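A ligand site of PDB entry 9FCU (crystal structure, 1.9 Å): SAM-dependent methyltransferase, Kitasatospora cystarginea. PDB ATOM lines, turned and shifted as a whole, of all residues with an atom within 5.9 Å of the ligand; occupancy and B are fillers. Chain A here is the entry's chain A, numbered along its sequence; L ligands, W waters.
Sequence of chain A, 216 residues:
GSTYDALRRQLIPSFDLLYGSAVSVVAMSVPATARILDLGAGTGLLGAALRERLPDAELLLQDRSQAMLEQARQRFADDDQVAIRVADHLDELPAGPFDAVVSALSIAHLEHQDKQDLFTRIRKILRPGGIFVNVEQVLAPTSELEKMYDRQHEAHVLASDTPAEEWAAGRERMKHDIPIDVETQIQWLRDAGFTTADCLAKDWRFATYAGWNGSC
The backbone carbonyl oxygen (O) of Leu 105 lies close to a sulfur (S1) of the ligand, 3.8 Å away. Gly 42 touches the ligand. Leu 45 touches the ligand (CB to O1, 3.8 Å). CB of Ser 65 touches O5 of the ligand, 3.6 Å away. Met 68 touches the ligand. O of Ala 87 touches C13 of the ligand, at 3.7 Å. ND1 of His 109 touches C10 of the ligand (3.9 Å). CD2 of Leu 110 touches N4 of the ligand, at 3.8 Å. Of the 27 residues printed, 17 come within 4 Å of the ligand.
OG of Ser 106 sits at hydrogen-bond distance from O3 of the ligand. O of Ala 104 is in hydrogen-bond range of N1 of the ligand, 2.8 Å away. N1 of the ligand lies close to O of Ala 41 (3.4 Å). The backbone NH of Arg 64 is in hydrogen-bond range of a nitrogen (N6) of the ligand (3.4 Å). The backbone NH (N) of His 89 sits at hydrogen-bond distance from a nitrogen (N5) of the ligand, at 2.9 Å. The backbone carbonyl oxygen (O) of Gly 40 lies within hydrogen-bond range of a nitrogen (N1) of the ligand. The side-chain carboxylate (OD2) of Asp 88 is in hydrogen-bond range of a nitrogen (N4) of the ligand. The side-chain hydroxyl of Tyr 19 sits at hydrogen-bond distance from an oxygen (O2) of the ligand, at 2.6 Å. An oxygen (O5) of the ligand is in hydrogen-bond range of the side-chain carboxylate (OD2) of Asp 63 (2.7 Å).
Water W3 lies within hydrogen-bond range of OG1 of Thr 43 (2.6 Å), O1 of the ligand (2.7 Å) and OH of Tyr 4 (2.8 Å). Water W1 bridges the guanidinium group of Arg 64 (2.6 Å) and an oxygen (O5) of the ligand (2.7 Å). Water W5 lies within hydrogen-bond range of the backbone carbonyl oxygen of Ala 41 (3.0 Å), the backbone NH of Leu 46 (3.1 Å), a nitrogen (N1) of the ligand (3.2 Å), the backbone NH of Leu 45 (3.4 Å) and the side-chain carboxylate of Asp 38 (3.5 Å). Water W4 lies within hydrogen-bond range of ND1 of His 89 (2.9 Å), O of Ala 87 (3.1 Å) and NE2 of Gln 62 (3.2 Å).
N of Arg 64 sits at hydrogen-bond distance from O of Ala 87, at 3.3 Å. The backbone carbonyl oxygen of Ser 106 sits at hydrogen-bond distance from a ring nitrogen (ND1) of His 109 (3.0 Å). The side-chain carboxylate (OD1) of Asp 63 lies within hydrogen-bond range of the backbone NH (N) of Ala 41 (3.4 Å). N of Gly 40 lies within hydrogen-bond range of O of Gln 62 (2.8 Å). The side-chain carboxylate of Asp 63 lies within hydrogen-bond range of the backbone NH of Gly 42, at 3.0 Å. N of Met 68 sits at hydrogen-bond distance from OG of Ser 65, at 3.1 Å. N of Leu 90 sits at hydrogen-bond distance from OD2 of Asp 88, at 3.0 Å. The backbone NH (N) of Ala 41 sits at hydrogen-bond distance from the backbone carbonyl oxygen (O) of Gln 62.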
ATOM      1  N   TYR A   4       3.351 -26.205 -16.795  1.00  0.00           N
ATOM      2  CA  TYR A   4       3.946 -25.098 -15.998  1.00  0.00           C
ATOM      3  C   TYR A   4       2.976 -24.705 -14.876  1.00  0.00           C
ATOM      4  O   TYR A   4       3.435 -24.512 -13.739  1.00  0.00           O
ATOM      5  CB  TYR A   4       4.279 -23.916 -16.931  1.00  0.00           C
ATOM      6  CG  TYR A   4       4.739 -22.661 -16.230  1.00  0.00           C
ATOM      7  CD1 TYR A   4       6.079 -22.363 -16.098  1.00  0.00           C
ATOM      8  CD2 TYR A   4       3.817 -21.767 -15.706  1.00  0.00           C
ATOM      9  CE1 TYR A   4       6.512 -21.204 -15.463  1.00  0.00           C
ATOM     10  CE2 TYR A   4       4.234 -20.604 -15.056  1.00  0.00           C
ATOM     11  CZ  TYR A   4       5.579 -20.329 -14.945  1.00  0.00           C
ATOM     12  OH  TYR A   4       5.988 -19.191 -14.308  1.00  0.00           O
ATOM     13  N   ARG A   8       3.299 -24.502 -10.535  1.00  0.00           N
ATOM     14  CA  ARG A   8       3.057 -23.253  -9.764  1.00  0.00           C
ATOM     15  C   ARG A   8       2.123 -23.558  -8.594  1.00  0.00           C
ATOM     16  O   ARG A   8       2.395 -23.059  -7.484  1.00  0.00           O
ATOM     17  CB  ARG A   8       2.535 -22.135 -10.673  1.00  0.00           C
ATOM     18  CG  ARG A   8       3.462 -21.773 -11.822  1.00  0.00           C
ATOM     19  CD  ARG A   8       4.856 -21.369 -11.378  1.00  0.00           C
ATOM     20  NE  ARG A   8       4.854 -20.110 -10.642  1.00  0.00           N
ATOM     21  CZ  ARG A   8       5.878 -19.620  -9.952  1.00  0.00           C
ATOM     22  NH1 ARG A   8       7.024 -20.287  -9.893  1.00  0.00           N
ATOM     23  NH2 ARG A   8       5.760 -18.468  -9.327  1.00  0.00           N
ATOM     24  N   TYR A  19      -4.718 -16.302  -5.760  1.00  0.00           N
ATOM     25  CA  TYR A  19      -4.963 -15.784  -7.143  1.00  0.00           C
ATOM     26  C   TYR A  19      -6.463 -15.548  -7.337  1.00  0.00           C
ATOM     27  O   TYR A  19      -6.838 -14.524  -7.933  1.00  0.00           O
ATOM     28  CB  TYR A  19      -4.386 -16.729  -8.205  1.00  0.00           C
ATOM     29  CG  TYR A  19      -2.903 -16.599  -8.417  1.00  0.00           C
ATOM     30  CD1 TYR A  19      -2.390 -16.050  -9.590  1.00  0.00           C
ATOM     31  CD2 TYR A  19      -1.996 -17.006  -7.445  1.00  0.00           C
ATOM     32  CE1 TYR A  19      -1.022 -15.925  -9.795  1.00  0.00           C
ATOM     33  CE2 TYR A  19      -0.630 -16.893  -7.642  1.00  0.00           C
ATOM     34  CZ  TYR A  19      -0.137 -16.352  -8.821  1.00  0.00           C
ATOM     35  OH  TYR A  19       1.199 -16.236  -9.024  1.00  0.00           O
ATOM     36  N   ASP A  38      -0.906  -5.416 -15.722  1.00  0.00           N
ATOM     37  CA  ASP A  38      -0.350  -6.593 -15.011  1.00  0.00           C
ATOM     38  C   ASP A  38       1.172  -6.454 -14.970  1.00  0.00           C
ATOM     39  O   ASP A  38       1.818  -6.707 -16.000  1.00  0.00           O
ATOM     40  CB  ASP A  38      -0.823  -7.879 -15.711  1.00  0.00           C
ATOM     41  CG  ASP A  38      -0.486  -9.170 -14.984  1.00  0.00           C
ATOM     42  OD1 ASP A  38       0.134  -9.109 -13.903  1.00  0.00           O
ATOM     43  OD2 ASP A  38      -0.835 -10.231 -15.521  1.00  0.00           O
ATOM     44  N   LEU A  39       1.716  -6.021 -13.818  1.00  0.00           N
ATOM     45  CA  LEU A  39       3.166  -5.751 -13.613  1.00  0.00           C
ATOM     46  C   LEU A  39       3.911  -7.048 -13.286  1.00  0.00           C
ATOM     47  O   LEU A  39       3.493  -7.744 -12.334  1.00  0.00           O
ATOM     48  CB  LEU A  39       3.348  -4.744 -12.463  1.00  0.00           C
ATOM     49  CG  LEU A  39       2.796  -3.340 -12.706  1.00  0.00           C
ATOM     50  CD1 LEU A  39       3.000  -2.474 -11.475  1.00  0.00           C
ATOM     51  CD2 LEU A  39       3.429  -2.706 -13.931  1.00  0.00           C
ATOM     52  N   GLY A  40       4.994  -7.333 -14.008  1.00  0.00           N
ATOM     53  CA  GLY A  40       5.760  -8.580 -13.861  1.00  0.00           C
ATOM     54  C   GLY A  40       4.892  -9.784 -14.185  1.00  0.00           C
ATOM     55  O   GLY A  40       4.891 -10.751 -13.392  1.00  0.00           O
ATOM     56  N   ALA A  41       4.162  -9.705 -15.300  1.00  0.00           N
ATOM     57  CA  ALA A  41       3.087 -10.647 -15.712  1.00  0.00           C
ATOM     58  C   ALA A  41       3.651 -12.059 -15.902  1.00  0.00           C
ATOM     59  O   ALA A  41       2.863 -13.018 -15.728  1.00  0.00           O
ATOM     60  CB  ALA A  41       2.437 -10.152 -16.978  1.00  0.00           C
ATOM     61  N   GLY A  42       4.944 -12.183 -16.237  1.00  0.00           N
ATOM     62  CA  GLY A  42       5.594 -13.473 -16.500  1.00  0.00           C
ATOM     63  C   GLY A  42       4.896 -14.187 -17.649  1.00  0.00           C
ATOM     64  O   GLY A  42       4.747 -13.565 -18.722  1.00  0.00           O
ATOM     65  N   THR A  43       4.442 -15.420 -17.416  1.00  0.00           N
ATOM     66  CA  THR A  43       3.698 -16.250 -18.404  1.00  0.00           C
ATOM     67  C   THR A  43       2.228 -15.805 -18.465  1.00  0.00           C
ATOM     68  O   THR A  43       1.493 -16.371 -19.305  1.00  0.00           O
ATOM     69  CB  THR A  43       3.796 -17.748 -18.090  1.00  0.00           C
ATOM     70  OG1 THR A  43       3.031 -18.019 -16.917  1.00  0.00           O
ATOM     71  CG2 THR A  43       5.224 -18.223 -17.905  1.00  0.00           C
ATOM     72  N   GLY A  44       1.811 -14.867 -17.611  1.00  0.00           N
ATOM     73  CA  GLY A  44       0.478 -14.229 -17.671  1.00  0.00           C
ATOM     74  C   GLY A  44      -0.576 -15.019 -16.905  1.00  0.00           C
ATOM     75  O   GLY A  44      -1.750 -14.983 -17.312  1.00  0.00           O
ATOM     76  N   LEU A  45      -0.175 -15.686 -15.818  1.00  0.00           N
ATOM     77  CA  LEU A  45      -1.026 -16.636 -15.060  1.00  0.00           C
ATOM     78  C   LEU A  45      -2.179 -15.888 -14.376  1.00  0.00           C
ATOM     79  O   LEU A  45      -3.336 -16.338 -14.507  1.00  0.00           O
ATOM     80  CB  LEU A  45      -0.146 -17.376 -14.041  1.00  0.00           C
ATOM     81  CG  LEU A  45      -0.734 -18.647 -13.438  1.00  0.00           C
ATOM     82  CD1 LEU A  45      -1.306 -19.562 -14.511  1.00  0.00           C
ATOM     83  CD2 LEU A  45       0.338 -19.385 -12.629  1.00  0.00           C
ATOM     84  N   LEU A  46      -1.899 -14.778 -13.681  1.00  0.00           N
ATOM     85  CA  LEU A  46      -2.956 -13.947 -13.048  1.00  0.00           C
ATOM     86  C   LEU A  46      -3.804 -13.281 -14.130  1.00  0.00           C
ATOM     87  O   LEU A  46      -5.030 -13.190 -13.954  1.00  0.00           O
ATOM     88  CB  LEU A  46      -2.313 -12.912 -12.110  1.00  0.00           C
ATOM     89  CG  LEU A  46      -3.308 -11.963 -11.420  1.00  0.00           C
ATOM     90  CD1 LEU A  46      -4.357 -12.740 -10.634  1.00  0.00           C
ATOM     91  CD2 LEU A  46      -2.583 -10.980 -10.506  1.00  0.00           C
ATOM     92  N   GLN A  62       2.975  -6.598 -18.715  1.00  0.00           N
ATOM     93  CA  GLN A  62       4.295  -5.915 -18.671  1.00  0.00           C
ATOM     94  C   GLN A  62       5.286  -6.777 -17.882  1.00  0.00           C
ATOM     95  O   GLN A  62       4.891  -7.306 -16.837  1.00  0.00           O
ATOM     96  CB  GLN A  62       4.108  -4.542 -18.020  1.00  0.00           C
ATOM     97  CG  GLN A  62       5.362  -3.699 -18.055  1.00  0.00           C
ATOM     98  CD  GLN A  62       5.062  -2.279 -17.646  1.00  0.00           C
ATOM     99  OE1 GLN A  62       4.272  -1.592 -18.293  1.00  0.00           O
ATOM    100  NE2 GLN A  62       5.683  -1.835 -16.569  1.00  0.00           N
ATOM    101  N   ASP A  63       6.532  -6.891 -18.378  1.00  0.00           N
ATOM    102  CA  ASP A  63       7.632  -7.647 -17.733  1.00  0.00           C
ATOM    103  C   ASP A  63       8.963  -7.211 -18.342  1.00  0.00           C
ATOM    104  O   ASP A  63       8.965  -6.774 -19.503  1.00  0.00           O
ATOM    105  CB  ASP A  63       7.398  -9.158 -17.881  1.00  0.00           C
ATOM    106  CG  ASP A  63       8.080  -9.985 -16.812  1.00  0.00           C
ATOM    107  OD1 ASP A  63       7.360 -10.490 -15.919  1.00  0.00           O
ATOM    108  OD2 ASP A  63       9.318 -10.142 -16.888  1.00  0.00           O
ATOM    109  N   ARG A  64      10.056  -7.333 -17.581  1.00  0.00           N
ATOM    110  CA  ARG A  64      11.427  -7.023 -18.067  1.00  0.00           C
ATOM    111  C   ARG A  64      11.942  -8.183 -18.928  1.00  0.00           C
ATOM    112  O   ARG A  64      12.837  -7.939 -19.768  1.00  0.00           O
ATOM    113  CB  ARG A  64      12.388  -6.736 -16.906  1.00  0.00           C
ATOM    114  CG  ARG A  64      12.678  -7.922 -15.996  1.00  0.00           C
ATOM    115  CD  ARG A  64      13.894  -7.699 -15.125  1.00  0.00           C
ATOM    116  NE  ARG A  64      14.064  -8.804 -14.181  1.00  0.00           N
ATOM    117  CZ  ARG A  64      14.701  -8.739 -13.009  1.00  0.00           C
ATOM    118  NH1 ARG A  64      15.246  -7.610 -12.592  1.00  0.00           N
ATOM    119  NH2 ARG A  64      14.779  -9.816 -12.252  1.00  0.00           N
ATOM    120  N   SER A  65      11.423  -9.406 -18.741  1.00  0.00           N
ATOM    121  CA  SER A  65      11.912 -10.640 -19.407  1.00  0.00           C
ATOM    122  C   SER A  65      11.074 -10.941 -20.667  1.00  0.00           C
ATOM    123  O   SER A  65       9.897 -11.310 -20.523  1.00  0.00           O
ATOM    124  CB  SER A  65      11.908 -11.819 -18.465  1.00  0.00           C
ATOM    125  OG  SER A  65      12.189 -13.016 -19.184  1.00  0.00           O
ATOM    126  N   MET A  68       9.998 -14.742 -20.613  1.00  0.00           N
ATOM    127  CA  MET A  68       8.745 -14.976 -19.838  1.00  0.00           C
ATOM    128  C   MET A  68       7.540 -14.548 -20.679  1.00  0.00           C
ATOM    129  O   MET A  68       6.581 -15.331 -20.770  1.00  0.00           O
ATOM    130  CB  MET A  68       8.768 -14.212 -18.508  1.00  0.00           C
ATOM    131  CG  MET A  68       9.795 -14.740 -17.511  1.00  0.00           C
ATOM    132  SD  MET A  68       9.462 -16.435 -16.960  1.00  0.00           S
ATOM    133  CE  MET A  68       8.045 -16.173 -15.885  1.00  0.00           C
ATOM    134  N   ALA A  87       9.123  -3.904 -20.205  1.00  0.00           N
ATOM    135  CA  ALA A  87       9.494  -2.775 -19.332  1.00  0.00           C
ATOM    136  C   ALA A  87       9.813  -3.268 -17.912  1.00  0.00           C
ATOM    137  O   ALA A  87       9.154  -4.207 -17.428  1.00  0.00           O
ATOM    138  CB  ALA A  87       8.381  -1.755 -19.325  1.00  0.00           C
ATOM    139  N   ASP A  88      10.806  -2.625 -17.288  1.00  0.00           N
ATOM    140  CA  ASP A  88      11.166  -2.813 -15.858  1.00  0.00           C
ATOM    141  C   ASP A  88      10.166  -2.040 -14.992  1.00  0.00           C
ATOM    142  O   ASP A  88       9.685  -0.989 -15.463  1.00  0.00           O
ATOM    143  CB  ASP A  88      12.610  -2.362 -15.616  1.00  0.00           C
ATOM    144  CG  ASP A  88      13.216  -2.960 -14.352  1.00  0.00           C
ATOM    145  OD1 ASP A  88      14.117  -3.805 -14.479  1.00  0.00           O
ATOM    146  OD2 ASP A  88      12.783  -2.563 -13.254  1.00  0.00           O
ATOM    147  N   HIS A  89       9.874  -2.520 -13.785  1.00  0.00           N
ATOM    148  CA  HIS A  89       9.042  -1.821 -12.764  1.00  0.00           C
ATOM    149  C   HIS A  89       9.617  -0.421 -12.513  1.00  0.00           C
ATOM    150  O   HIS A  89       8.826   0.487 -12.174  1.00  0.00           O
ATOM    151  CB  HIS A  89       9.006  -2.570 -11.422  1.00  0.00           C
ATOM    152  CG  HIS A  89       8.453  -3.947 -11.484  1.00  0.00           C
ATOM    153  ND1 HIS A  89       7.488  -4.326 -12.379  1.00  0.00           N
ATOM    154  CD2 HIS A  89       8.708  -5.030 -10.716  1.00  0.00           C
ATOM    155  CE1 HIS A  89       7.179  -5.592 -12.189  1.00  0.00           C
ATOM    156  NE2 HIS A  89       7.916  -6.044 -11.171  1.00  0.00           N
ATOM    157  N   LEU A  90      10.943  -0.269 -12.638  1.00  0.00           N
ATOM    158  CA  LEU A  90      11.696   0.976 -12.329  1.00  0.00           C
ATOM    159  C   LEU A  90      11.605   1.966 -13.501  1.00  0.00           C
ATOM    160  O   LEU A  90      11.841   3.160 -13.259  1.00  0.00           O
ATOM    161  CB  LEU A  90      13.150   0.605 -12.029  1.00  0.00           C
ATOM    162  CG  LEU A  90      13.361  -0.339 -10.837  1.00  0.00           C
ATOM    163  CD1 LEU A  90      14.835  -0.653 -10.653  1.00  0.00           C
ATOM    164  CD2 LEU A  90      12.781   0.245  -9.566  1.00  0.00           C
ATOM    165  N   SER A 103      -0.426  -7.433  -9.731  1.00  0.00           N
ATOM    166  CA  SER A 103       0.924  -8.036  -9.729  1.00  0.00           C
ATOM    167  C   SER A 103       0.898  -9.306  -8.883  1.00  0.00           C
ATOM    168  O   SER A 103       0.141  -9.342  -7.887  1.00  0.00           O
ATOM    169  CB  SER A 103       1.962  -7.044  -9.253  1.00  0.00           C
ATOM    170  OG  SER A 103       3.274  -7.496  -9.572  1.00  0.00           O
ATOM    171  N   ALA A 104       1.632 -10.325  -9.307  1.00  0.00           N
ATOM    172  CA  ALA A 104       1.787 -11.605  -8.599  1.00  0.00           C
ATOM    173  C   ALA A 104       3.266 -11.986  -8.583  1.00  0.00           C
ATOM    174  O   ALA A 104       3.840 -12.132  -9.682  1.00  0.00           O
ATOM    175  CB  ALA A 104       0.952 -12.680  -9.255  1.00  0.00           C
ATOM    176  N   LEU A 105       3.850 -12.070  -7.367  1.00  0.00           N
ATOM    177  CA  LEU A 105       5.171 -12.686  -7.066  1.00  0.00           C
ATOM    178  C   LEU A 105       6.294 -11.995  -7.854  1.00  0.00           C
ATOM    179  O   LEU A 105       7.234 -12.699  -8.264  1.00  0.00           O
ATOM    180  CB  LEU A 105       5.102 -14.191  -7.386  1.00  0.00           C
ATOM    181  CG  LEU A 105       4.045 -14.993  -6.627  1.00  0.00           C
ATOM    182  CD1 LEU A 105       4.143 -16.476  -6.951  1.00  0.00           C
ATOM    183  CD2 LEU A 105       4.167 -14.772  -5.124  1.00  0.00           C
ATOM    184  N   SER A 106       6.232 -10.676  -7.995  1.00  0.00           N
ATOM    185  CA  SER A 106       7.179  -9.875  -8.819  1.00  0.00           C
ATOM    186  C   SER A 106       7.827  -8.750  -7.990  1.00  0.00           C
ATOM    187  O   SER A 106       9.053  -8.572  -8.096  1.00  0.00           O
ATOM    188  CB  SER A 106       6.501  -9.312 -10.028  1.00  0.00           C
ATOM    189  OG  SER A 106       7.460  -8.796 -10.943  1.00  0.00           O
ATOM    190  N   HIS A 109      11.054  -8.549  -5.592  1.00  0.00           N
ATOM    191  CA  HIS A 109      12.416  -8.504  -6.213  1.00  0.00           C
ATOM    192  C   HIS A 109      13.044  -7.102  -6.099  1.00  0.00           C
ATOM    193  O   HIS A 109      14.264  -7.013  -6.238  1.00  0.00           O
ATOM    194  CB  HIS A 109      12.383  -8.948  -7.686  1.00  0.00           C
ATOM    195  CG  HIS A 109      12.165 -10.418  -7.857  1.00  0.00           C
ATOM    196  ND1 HIS A 109      10.940 -10.948  -8.201  1.00  0.00           N
ATOM    197  CD2 HIS A 109      13.010 -11.466  -7.734  1.00  0.00           C
ATOM    198  CE1 HIS A 109      11.041 -12.257  -8.282  1.00  0.00           C
ATOM    199  NE2 HIS A 109      12.298 -12.601  -8.006  1.00  0.00           N
ATOM    200  N   LEU A 110      12.233  -6.060  -5.877  1.00  0.00           N
ATOM    201  CA  LEU A 110      12.725  -4.653  -5.763  1.00  0.00           C
ATOM    202  C   LEU A 110      13.254  -4.407  -4.348  1.00  0.00           C
ATOM    203  O   LEU A 110      12.734  -5.031  -3.399  1.00  0.00           O
ATOM    204  CB  LEU A 110      11.584  -3.678  -6.071  1.00  0.00           C
ATOM    205  CG  LEU A 110      11.009  -3.731  -7.481  1.00  0.00           C
ATOM    206  CD1 LEU A 110       9.869  -2.740  -7.620  1.00  0.00           C
ATOM    207  CD2 LEU A 110      12.083  -3.468  -8.523  1.00  0.00           C
HETATM  208  N1  LIG L   1       3.335 -12.927 -12.343  1.00  0.00           N
HETATM  209  C1  LIG L   1       3.720 -14.283 -12.822  1.00  0.00           C
HETATM  210  C2  LIG L   1       5.239 -14.481 -12.800  1.00  0.00           C
HETATM  211  C3  LIG L   1       5.871 -14.359 -11.423  1.00  0.00           C
HETATM  212  S1  LIG L   1       7.667 -14.625 -11.479  1.00  0.00           S
HETATM  213  C4  LIG L   1       3.039 -15.360 -11.964  1.00  0.00           C
HETATM  214  O1  LIG L   1       3.142 -16.541 -12.283  1.00  0.00           O
HETATM  215  O2  LIG L   1       2.383 -15.068 -10.970  1.00  0.00           O
HETATM  216  C5  LIG L   1       8.318 -12.953 -11.311  1.00  0.00           C
HETATM  217  C6  LIG L   1       8.276 -12.151 -12.587  1.00  0.00           C
HETATM  218  O3  LIG L   1       8.685 -10.801 -12.296  1.00  0.00           O
HETATM  219  C7  LIG L   1       9.212 -12.658 -13.697  1.00  0.00           C
HETATM  220  O4  LIG L   1       8.492 -12.755 -14.920  1.00  0.00           O
HETATM  221  C8  LIG L   1      10.312 -11.592 -13.758  1.00  0.00           C
HETATM  222  O5  LIG L   1      10.849 -11.421 -15.056  1.00  0.00           O
HETATM  223  C9  LIG L   1       9.537 -10.356 -13.330  1.00  0.00           C
HETATM  224  N2  LIG L   1      10.342  -9.258 -12.807  1.00  0.00           N
HETATM  225  C10 LIG L   1      11.232  -9.299 -11.767  1.00  0.00           C
HETATM  226  N3  LIG L   1      11.776  -8.139 -11.500  1.00  0.00           N
HETATM  227  C11 LIG L   1      11.196  -7.276 -12.413  1.00  0.00           C
HETATM  228  C12 LIG L   1      11.348  -5.892 -12.646  1.00  0.00           C
HETATM  229  N4  LIG L   1      12.161  -5.108 -11.931  1.00  0.00           N
HETATM  230  N5  LIG L   1      10.611  -5.330 -13.626  1.00  0.00           N
HETATM  231  C13 LIG L   1       9.790  -6.121 -14.341  1.00  0.00           C
HETATM  232  N6  LIG L   1       9.558  -7.422 -14.218  1.00  0.00           N
HETATM  233  C14 LIG L   1      10.305  -7.948 -13.219  1.00  0.00           C
HETATM  234  O   HOH W   1      13.566 -11.169 -15.046  1.00  0.00           O
HETATM  235  O   HOH W   2       2.064 -10.116 -12.244  1.00  0.00           O
HETATM  236  O   HOH W   3       4.178 -17.035 -14.753  1.00  0.00           O
HETATM  237  O   HOH W   4       6.973  -4.483 -15.236  1.00  0.00           O
HETATM  238  O   HOH W   5       0.567 -12.959 -13.851  1.00  0.00           O
